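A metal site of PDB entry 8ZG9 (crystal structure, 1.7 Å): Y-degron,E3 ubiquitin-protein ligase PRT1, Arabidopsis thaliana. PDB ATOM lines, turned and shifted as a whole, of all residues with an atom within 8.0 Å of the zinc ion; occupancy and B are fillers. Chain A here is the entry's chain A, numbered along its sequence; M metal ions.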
ATOM      1  N   ARG A  28       4.736   8.590  -6.598  1.00  0.00           N
ATOM      2  CA  ARG A  28       3.296   8.703  -6.778  1.00  0.00           C
ATOM      3  C   ARG A  28       2.716   7.360  -7.179  1.00  0.00           C
ATOM      4  O   ARG A  28       3.326   6.611  -7.954  1.00  0.00           O
ATOM      5  CB  ARG A  28       2.985   9.745  -7.834  1.00  0.00           C
ATOM      6  CG  ARG A  28       1.545   9.736  -8.338  1.00  0.00           C
ATOM      7  CD  ARG A  28       1.322  10.883  -9.288  1.00  0.00           C
ATOM      8  NE  ARG A  28       2.325  10.909 -10.341  1.00  0.00           N
ATOM      9  CZ  ARG A  28       2.582  11.969 -11.107  1.00  0.00           C
ATOM     10  NH1 ARG A  28       1.910  13.098 -10.920  1.00  0.00           N
ATOM     11  NH2 ARG A  28       3.521  11.909 -12.045  1.00  0.00           N
ATOM     12  N   CYS A  29       1.551   7.042  -6.628  1.00  0.00           N
ATOM     13  CA  CYS A  29       0.856   5.809  -6.948  1.00  0.00           C
ATOM     14  C   CYS A  29       0.160   5.942  -8.298  1.00  0.00           C
ATOM     15  O   CYS A  29      -0.556   6.919  -8.551  1.00  0.00           O
ATOM     16  CB  CYS A  29      -0.152   5.452  -5.875  1.00  0.00           C
ATOM     17  SG  CYS A  29      -0.929   3.838  -6.128  1.00  0.00           S
ATOM     18  N   LYS A  30       0.387   4.939  -9.147  1.00  0.00           N
ATOM     19  CA  LYS A  30      -0.160   4.865 -10.484  1.00  0.00           C
ATOM     20  C   LYS A  30      -1.539   4.220 -10.526  1.00  0.00           C
ATOM     21  O   LYS A  30      -2.262   4.409 -11.503  1.00  0.00           O
ATOM     22  CB  LYS A  30       0.767   4.023 -11.369  1.00  0.00           C
ATOM     23  CG  LYS A  30       2.154   4.559 -11.540  1.00  0.00           C
ATOM     24  CD  LYS A  30       2.976   3.483 -12.200  1.00  0.00           C
ATOM     25  CE  LYS A  30       2.512   3.174 -13.597  1.00  0.00           C
ATOM     26  NZ  LYS A  30       3.256   2.039 -14.178  1.00  0.00           N
ATOM     27  N   ASP A  31      -1.908   3.496  -9.465  1.00  0.00           N
ATOM     28  CA  ASP A  31      -3.137   2.725  -9.437  1.00  0.00           C
ATOM     29  C   ASP A  31      -4.240   3.299  -8.545  1.00  0.00           C
ATOM     30  O   ASP A  31      -5.379   2.842  -8.644  1.00  0.00           O
ATOM     31  CB  ASP A  31      -2.785   1.285  -9.015  1.00  0.00           C
ATOM     32  CG  ASP A  31      -1.850   0.639 -10.004  1.00  0.00           C
ATOM     33  OD1 ASP A  31      -2.038   0.855 -11.214  1.00  0.00           O
ATOM     34  OD2 ASP A  31      -0.911  -0.059  -9.575  1.00  0.00           O
ATOM     35  N   CYS A  32      -3.932   4.251  -7.657  1.00  0.00           N
ATOM     36  CA  CYS A  32      -4.992   4.826  -6.824  1.00  0.00           C
ATOM     37  C   CYS A  32      -5.952   5.593  -7.725  1.00  0.00           C
ATOM     38  O   CYS A  32      -5.534   6.410  -8.547  1.00  0.00           O
ATOM     39  CB  CYS A  32      -4.399   5.736  -5.765  1.00  0.00           C
ATOM     40  SG  CYS A  32      -4.107   4.898  -4.203  1.00  0.00           S
ATOM     41  N   LYS A  33      -7.253   5.309  -7.583  1.00  0.00           N
ATOM     42  CA  LYS A  33      -8.276   5.886  -8.456  1.00  0.00           C
ATOM     43  C   LYS A  33      -8.841   7.185  -7.914  1.00  0.00           C
ATOM     44  O   LYS A  33      -9.485   7.932  -8.668  1.00  0.00           O
ATOM     45  CB  LYS A  33      -9.405   4.861  -8.655  1.00  0.00           C
ATOM     46  CG  LYS A  33      -8.977   3.571  -9.368  1.00  0.00           C
ATOM     47  CD  LYS A  33     -10.158   2.643  -9.620  1.00  0.00           C
ATOM     48  CE  LYS A  33     -10.672   2.042  -8.313  1.00  0.00           C
ATOM     49  NZ  LYS A  33      -9.694   1.100  -7.714  1.00  0.00           N
ATOM     50  N   GLU A  34      -8.616   7.480  -6.642  1.00  0.00           N
ATOM     51  CA  GLU A  34      -9.071   8.732  -6.052  1.00  0.00           C
ATOM     52  C   GLU A  34      -8.333   9.919  -6.662  1.00  0.00           C
ATOM     53  O   GLU A  34      -7.122   9.861  -6.935  1.00  0.00           O
ATOM     54  CB  GLU A  34      -8.898   8.661  -4.536  1.00  0.00           C
ATOM     55  CG  GLU A  34      -9.805   7.592  -3.951  1.00  0.00           C
ATOM     56  CD  GLU A  34      -9.170   6.200  -3.955  1.00  0.00           C
ATOM     57  OE1 GLU A  34      -8.048   6.039  -4.489  1.00  0.00           O
ATOM     58  OE2 GLU A  34      -9.782   5.266  -3.404  1.00  0.00           O
ATOM     59  N   GLY A  37      -5.171  11.328  -5.320  1.00  0.00           N
ATOM     60  CA  GLY A  37      -3.963  10.564  -5.527  1.00  0.00           C
ATOM     61  C   GLY A  37      -3.342  10.142  -4.217  1.00  0.00           C
ATOM     62  O   GLY A  37      -3.846  10.399  -3.134  1.00  0.00           O
ATOM     63  N   TYR A  38      -2.173   9.525  -4.338  1.00  0.00           N
ATOM     64  CA  TYR A  38      -1.434   8.975  -3.210  1.00  0.00           C
ATOM     65  C   TYR A  38       0.041   9.167  -3.487  1.00  0.00           C
ATOM     66  O   TYR A  38       0.500   8.918  -4.598  1.00  0.00           O
ATOM     67  CB  TYR A  38      -1.774   7.484  -3.009  1.00  0.00           C
ATOM     68  CG  TYR A  38      -1.071   6.813  -1.848  1.00  0.00           C
ATOM     69  CD1 TYR A  38       0.216   6.314  -1.990  1.00  0.00           C
ATOM     70  CD2 TYR A  38      -1.702   6.670  -0.625  1.00  0.00           C
ATOM     71  CE1 TYR A  38       0.850   5.699  -0.940  1.00  0.00           C
ATOM     72  CE2 TYR A  38      -1.055   6.055   0.443  1.00  0.00           C
ATOM     73  CZ  TYR A  38       0.213   5.574   0.275  1.00  0.00           C
ATOM     74  OH  TYR A  38       0.864   4.936   1.314  1.00  0.00           O
ATOM     75  N   ASP A  39       0.775   9.636  -2.482  1.00  0.00           N
ATOM     76  CA  ASP A  39       2.188   9.936  -2.672  1.00  0.00           C
ATOM     77  C   ASP A  39       2.971   9.624  -1.410  1.00  0.00           C
ATOM     78  O   ASP A  39       2.442   9.671  -0.299  1.00  0.00           O
ATOM     79  CB  ASP A  39       2.437  11.410  -3.033  1.00  0.00           C
ATOM     80  CG  ASP A  39       1.631  11.869  -4.221  1.00  0.00           C
ATOM     81  OD1 ASP A  39       0.463  12.249  -4.018  1.00  0.00           O
ATOM     82  OD2 ASP A  39       2.179  11.858  -5.340  1.00  0.00           O
ATOM     83  N   VAL A  51      -0.025   2.321   5.250  1.00  0.00           N
ATOM     84  CA  VAL A  51      -0.639   3.622   4.992  1.00  0.00           C
ATOM     85  C   VAL A  51      -1.623   3.496   3.835  1.00  0.00           C
ATOM     86  O   VAL A  51      -1.231   3.558   2.656  1.00  0.00           O
ATOM     87  CB  VAL A  51       0.427   4.688   4.712  1.00  0.00           C
ATOM     88  CG1 VAL A  51      -0.196   6.051   4.476  1.00  0.00           C
ATOM     89  CG2 VAL A  51       1.428   4.769   5.857  1.00  0.00           C
ATOM     90  N   PRO A  52      -2.927   3.311   4.110  1.00  0.00           N
ATOM     91  CA  PRO A  52      -3.914   3.382   3.023  1.00  0.00           C
ATOM     92  C   PRO A  52      -4.108   4.797   2.476  1.00  0.00           C
ATOM     93  O   PRO A  52      -4.550   4.946   1.324  1.00  0.00           O
ATOM     94  CB  PRO A  52      -5.207   2.865   3.683  1.00  0.00           C
ATOM     95  CG  PRO A  52      -5.017   3.080   5.142  1.00  0.00           C
ATOM     96  CD  PRO A  52      -3.531   2.946   5.400  1.00  0.00           C
ATOM     97  N   GLN A  57      -7.947   7.114   0.463  1.00  0.00           N
ATOM     98  CA  GLN A  57      -7.604   6.499  -0.816  1.00  0.00           C
ATOM     99  C   GLN A  57      -7.657   4.981  -0.817  1.00  0.00           C
ATOM    100  O   GLN A  57      -7.853   4.398  -1.883  1.00  0.00           O
ATOM    101  CB  GLN A  57      -6.207   6.953  -1.247  1.00  0.00           C
ATOM    102  CG  GLN A  57      -6.023   8.441  -1.389  1.00  0.00           C
ATOM    103  CD  GLN A  57      -5.402   9.056  -0.162  1.00  0.00           C
ATOM    104  OE1 GLN A  57      -5.835   8.810   0.957  1.00  0.00           O
ATOM    105  NE2 GLN A  57      -4.373   9.885  -0.361  1.00  0.00           N
ATOM    106  N   GLN A  58      -7.465   4.331   0.322  1.00  0.00           N
ATOM    107  CA  GLN A  58      -7.429   2.856   0.410  1.00  0.00           C
ATOM    108  C   GLN A  58      -6.372   2.258  -0.530  1.00  0.00           C
ATOM    109  O   GLN A  58      -6.605   1.278  -1.246  1.00  0.00           O
ATOM    110  CB  GLN A  58      -8.811   2.241   0.143  1.00  0.00           C
ATOM    111  CG  GLN A  58      -9.933   2.838   0.992  1.00  0.00           C
ATOM    112  CD  GLN A  58      -9.658   2.764   2.479  1.00  0.00           C
ATOM    113  OE1 GLN A  58      -9.021   1.836   2.965  1.00  0.00           O
ATOM    114  NE2 GLN A  58     -10.134   3.762   3.205  1.00  0.00           N
ATOM    115  N   HIS A  59      -5.192   2.881  -0.525  1.00  0.00           N
ATOM    116  CA  HIS A  59      -3.981   2.350  -1.148  1.00  0.00           C
ATOM    117  C   HIS A  59      -3.573   1.029  -0.509  1.00  0.00           C
ATOM    118  O   HIS A  59      -3.706   0.847   0.701  1.00  0.00           O
ATOM    119  CB  HIS A  59      -2.873   3.402  -0.978  1.00  0.00           C
ATOM    120  CG  HIS A  59      -1.532   3.009  -1.505  1.00  0.00           C
ATOM    121  ND1 HIS A  59      -1.205   3.086  -2.842  1.00  0.00           N
ATOM    122  CD2 HIS A  59      -0.420   2.588  -0.865  1.00  0.00           C
ATOM    123  CE1 HIS A  59       0.056   2.707  -3.001  1.00  0.00           C
ATOM    124  NE2 HIS A  59       0.546   2.394  -1.820  1.00  0.00           N
ATOM    125  N   THR A  60      -3.094   0.094  -1.333  1.00  0.00           N
ATOM    126  CA  THR A  60      -2.721  -1.229  -0.863  1.00  0.00           C
ATOM    127  C   THR A  60      -1.271  -1.547  -1.237  1.00  0.00           C
ATOM    128  O   THR A  60      -0.693  -0.875  -2.096  1.00  0.00           O
ATOM    129  CB  THR A  60      -3.592  -2.333  -1.473  1.00  0.00           C
ATOM    130  OG1 THR A  60      -3.238  -2.487  -2.847  1.00  0.00           O
ATOM    131  CG2 THR A  60      -5.033  -1.953  -1.393  1.00  0.00           C
ATOM    132  N   PRO A  61      -0.664  -2.559  -0.606  1.00  0.00           N
ATOM    133  CA  PRO A  61       0.720  -2.928  -0.971  1.00  0.00           C
ATOM    134  C   PRO A  61       0.868  -3.490  -2.380  1.00  0.00           C
ATOM    135  O   PRO A  61       2.008  -3.663  -2.821  1.00  0.00           O
ATOM    136  CB  PRO A  61       1.091  -4.005   0.065  1.00  0.00           C
ATOM    137  CG  PRO A  61       0.094  -3.834   1.181  1.00  0.00           C
ATOM    138  CD  PRO A  61      -1.167  -3.335   0.542  1.00  0.00           C
ATOM    139  N   ASP A  62      -0.231  -3.780  -3.086  1.00  0.00           N
ATOM    140  CA  ASP A  62      -0.167  -4.312  -4.440  1.00  0.00           C
ATOM    141  C   ASP A  62      -0.161  -3.228  -5.501  1.00  0.00           C
ATOM    142  O   ASP A  62       0.112  -3.535  -6.664  1.00  0.00           O
ATOM    143  CB  ASP A  62      -1.357  -5.241  -4.686  1.00  0.00           C
ATOM    144  CG  ASP A  62      -1.384  -6.425  -3.741  1.00  0.00           C
ATOM    145  OD1 ASP A  62      -0.403  -7.206  -3.733  1.00  0.00           O
ATOM    146  OD2 ASP A  62      -2.375  -6.564  -2.999  1.00  0.00           O
ATOM    147  N   HIS A  63      -0.472  -1.979  -5.137  1.00  0.00           N
ATOM    148  CA  HIS A  63      -0.418  -0.839  -6.045  1.00  0.00           C
ATOM    149  C   HIS A  63       1.037  -0.549  -6.452  1.00  0.00           C
ATOM    150  O   HIS A  63       1.984  -0.834  -5.713  1.00  0.00           O
ATOM    151  CB  HIS A  63      -1.013   0.406  -5.392  1.00  0.00           C
ATOM    152  CG  HIS A  63      -2.503   0.382  -5.268  1.00  0.00           C
ATOM    153  ND1 HIS A  63      -3.238   1.488  -4.897  1.00  0.00           N
ATOM    154  CD2 HIS A  63      -3.392  -0.608  -5.509  1.00  0.00           C
ATOM    155  CE1 HIS A  63      -4.523   1.150  -4.871  1.00  0.00           C
ATOM    156  NE2 HIS A  63      -4.643  -0.116  -5.249  1.00  0.00           N
ATOM    157  N   ARG A  64       1.185   0.045  -7.633  1.00  0.00           N
ATOM    158  CA  ARG A  64       2.491   0.371  -8.193  1.00  0.00           C
ATOM    159  C   ARG A  64       2.751   1.862  -8.060  1.00  0.00           C
ATOM    160  O   ARG A  64       1.903   2.692  -8.430  1.00  0.00           O
ATOM    161  CB  ARG A  64       2.557  -0.027  -9.662  1.00  0.00           C
ATOM    162  CG  ARG A  64       2.413  -1.504  -9.958  1.00  0.00           C
ATOM    163  CD  ARG A  64       2.186  -1.689 -11.452  1.00  0.00           C
ATOM    164  NE  ARG A  64       0.895  -1.149 -11.859  1.00  0.00           N
ATOM    165  CZ  ARG A  64       0.439  -1.144 -13.103  1.00  0.00           C
ATOM    166  NH1 ARG A  64       1.168  -1.660 -14.084  1.00  0.00           N
ATOM    167  NH2 ARG A  64      -0.751  -0.651 -13.373  1.00  0.00           N
ATOM    168  N   LEU A  65       3.919   2.197  -7.515  1.00  0.00           N
ATOM    169  CA  LEU A  65       4.397   3.554  -7.355  1.00  0.00           C
ATOM    170  C   LEU A  65       5.489   3.833  -8.383  1.00  0.00           C
ATOM    171  O   LEU A  65       6.137   2.907  -8.905  1.00  0.00           O
ATOM    172  CB  LEU A  65       4.952   3.759  -5.955  1.00  0.00           C
ATOM    173  CG  LEU A  65       3.975   3.524  -4.802  1.00  0.00           C
ATOM    174  CD1 LEU A  65       4.812   3.236  -3.551  1.00  0.00           C
ATOM    175  CD2 LEU A  65       2.995   4.651  -4.547  1.00  0.00           C
HETATM  176 ZN    ZN M   1      -2.388   3.427  -4.434  1.00  0.00          ZN
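ND1 of His 59 is bound to the zinc ion, 2.0 Å away. A ring nitrogen (ND1) of His 63 is bound to the zinc ion. The zinc ion is bound by SG of Cys 29, 2.3 Å away. The zinc ion is bound by the side-chain sulfur (SG) of Cys 32 (2.3 Å).
Of the 21 residues printed, 4 come within 4 Å of the zinc ion. The nearest printed residue that does not touch the zinc ion is Tyr 38 (4.3 Å).
SG of Cys 29 lies close to N of Asp 31, 3.5 Å away. The backbone NH (N) of Cys 29 is in hydrogen-bond range of the backbone carbonyl oxygen (O) of Tyr 38, 3.0 Å away. O of Pro 52 sits at hydrogen-bond distance from N of His 59 (2.8 Å).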
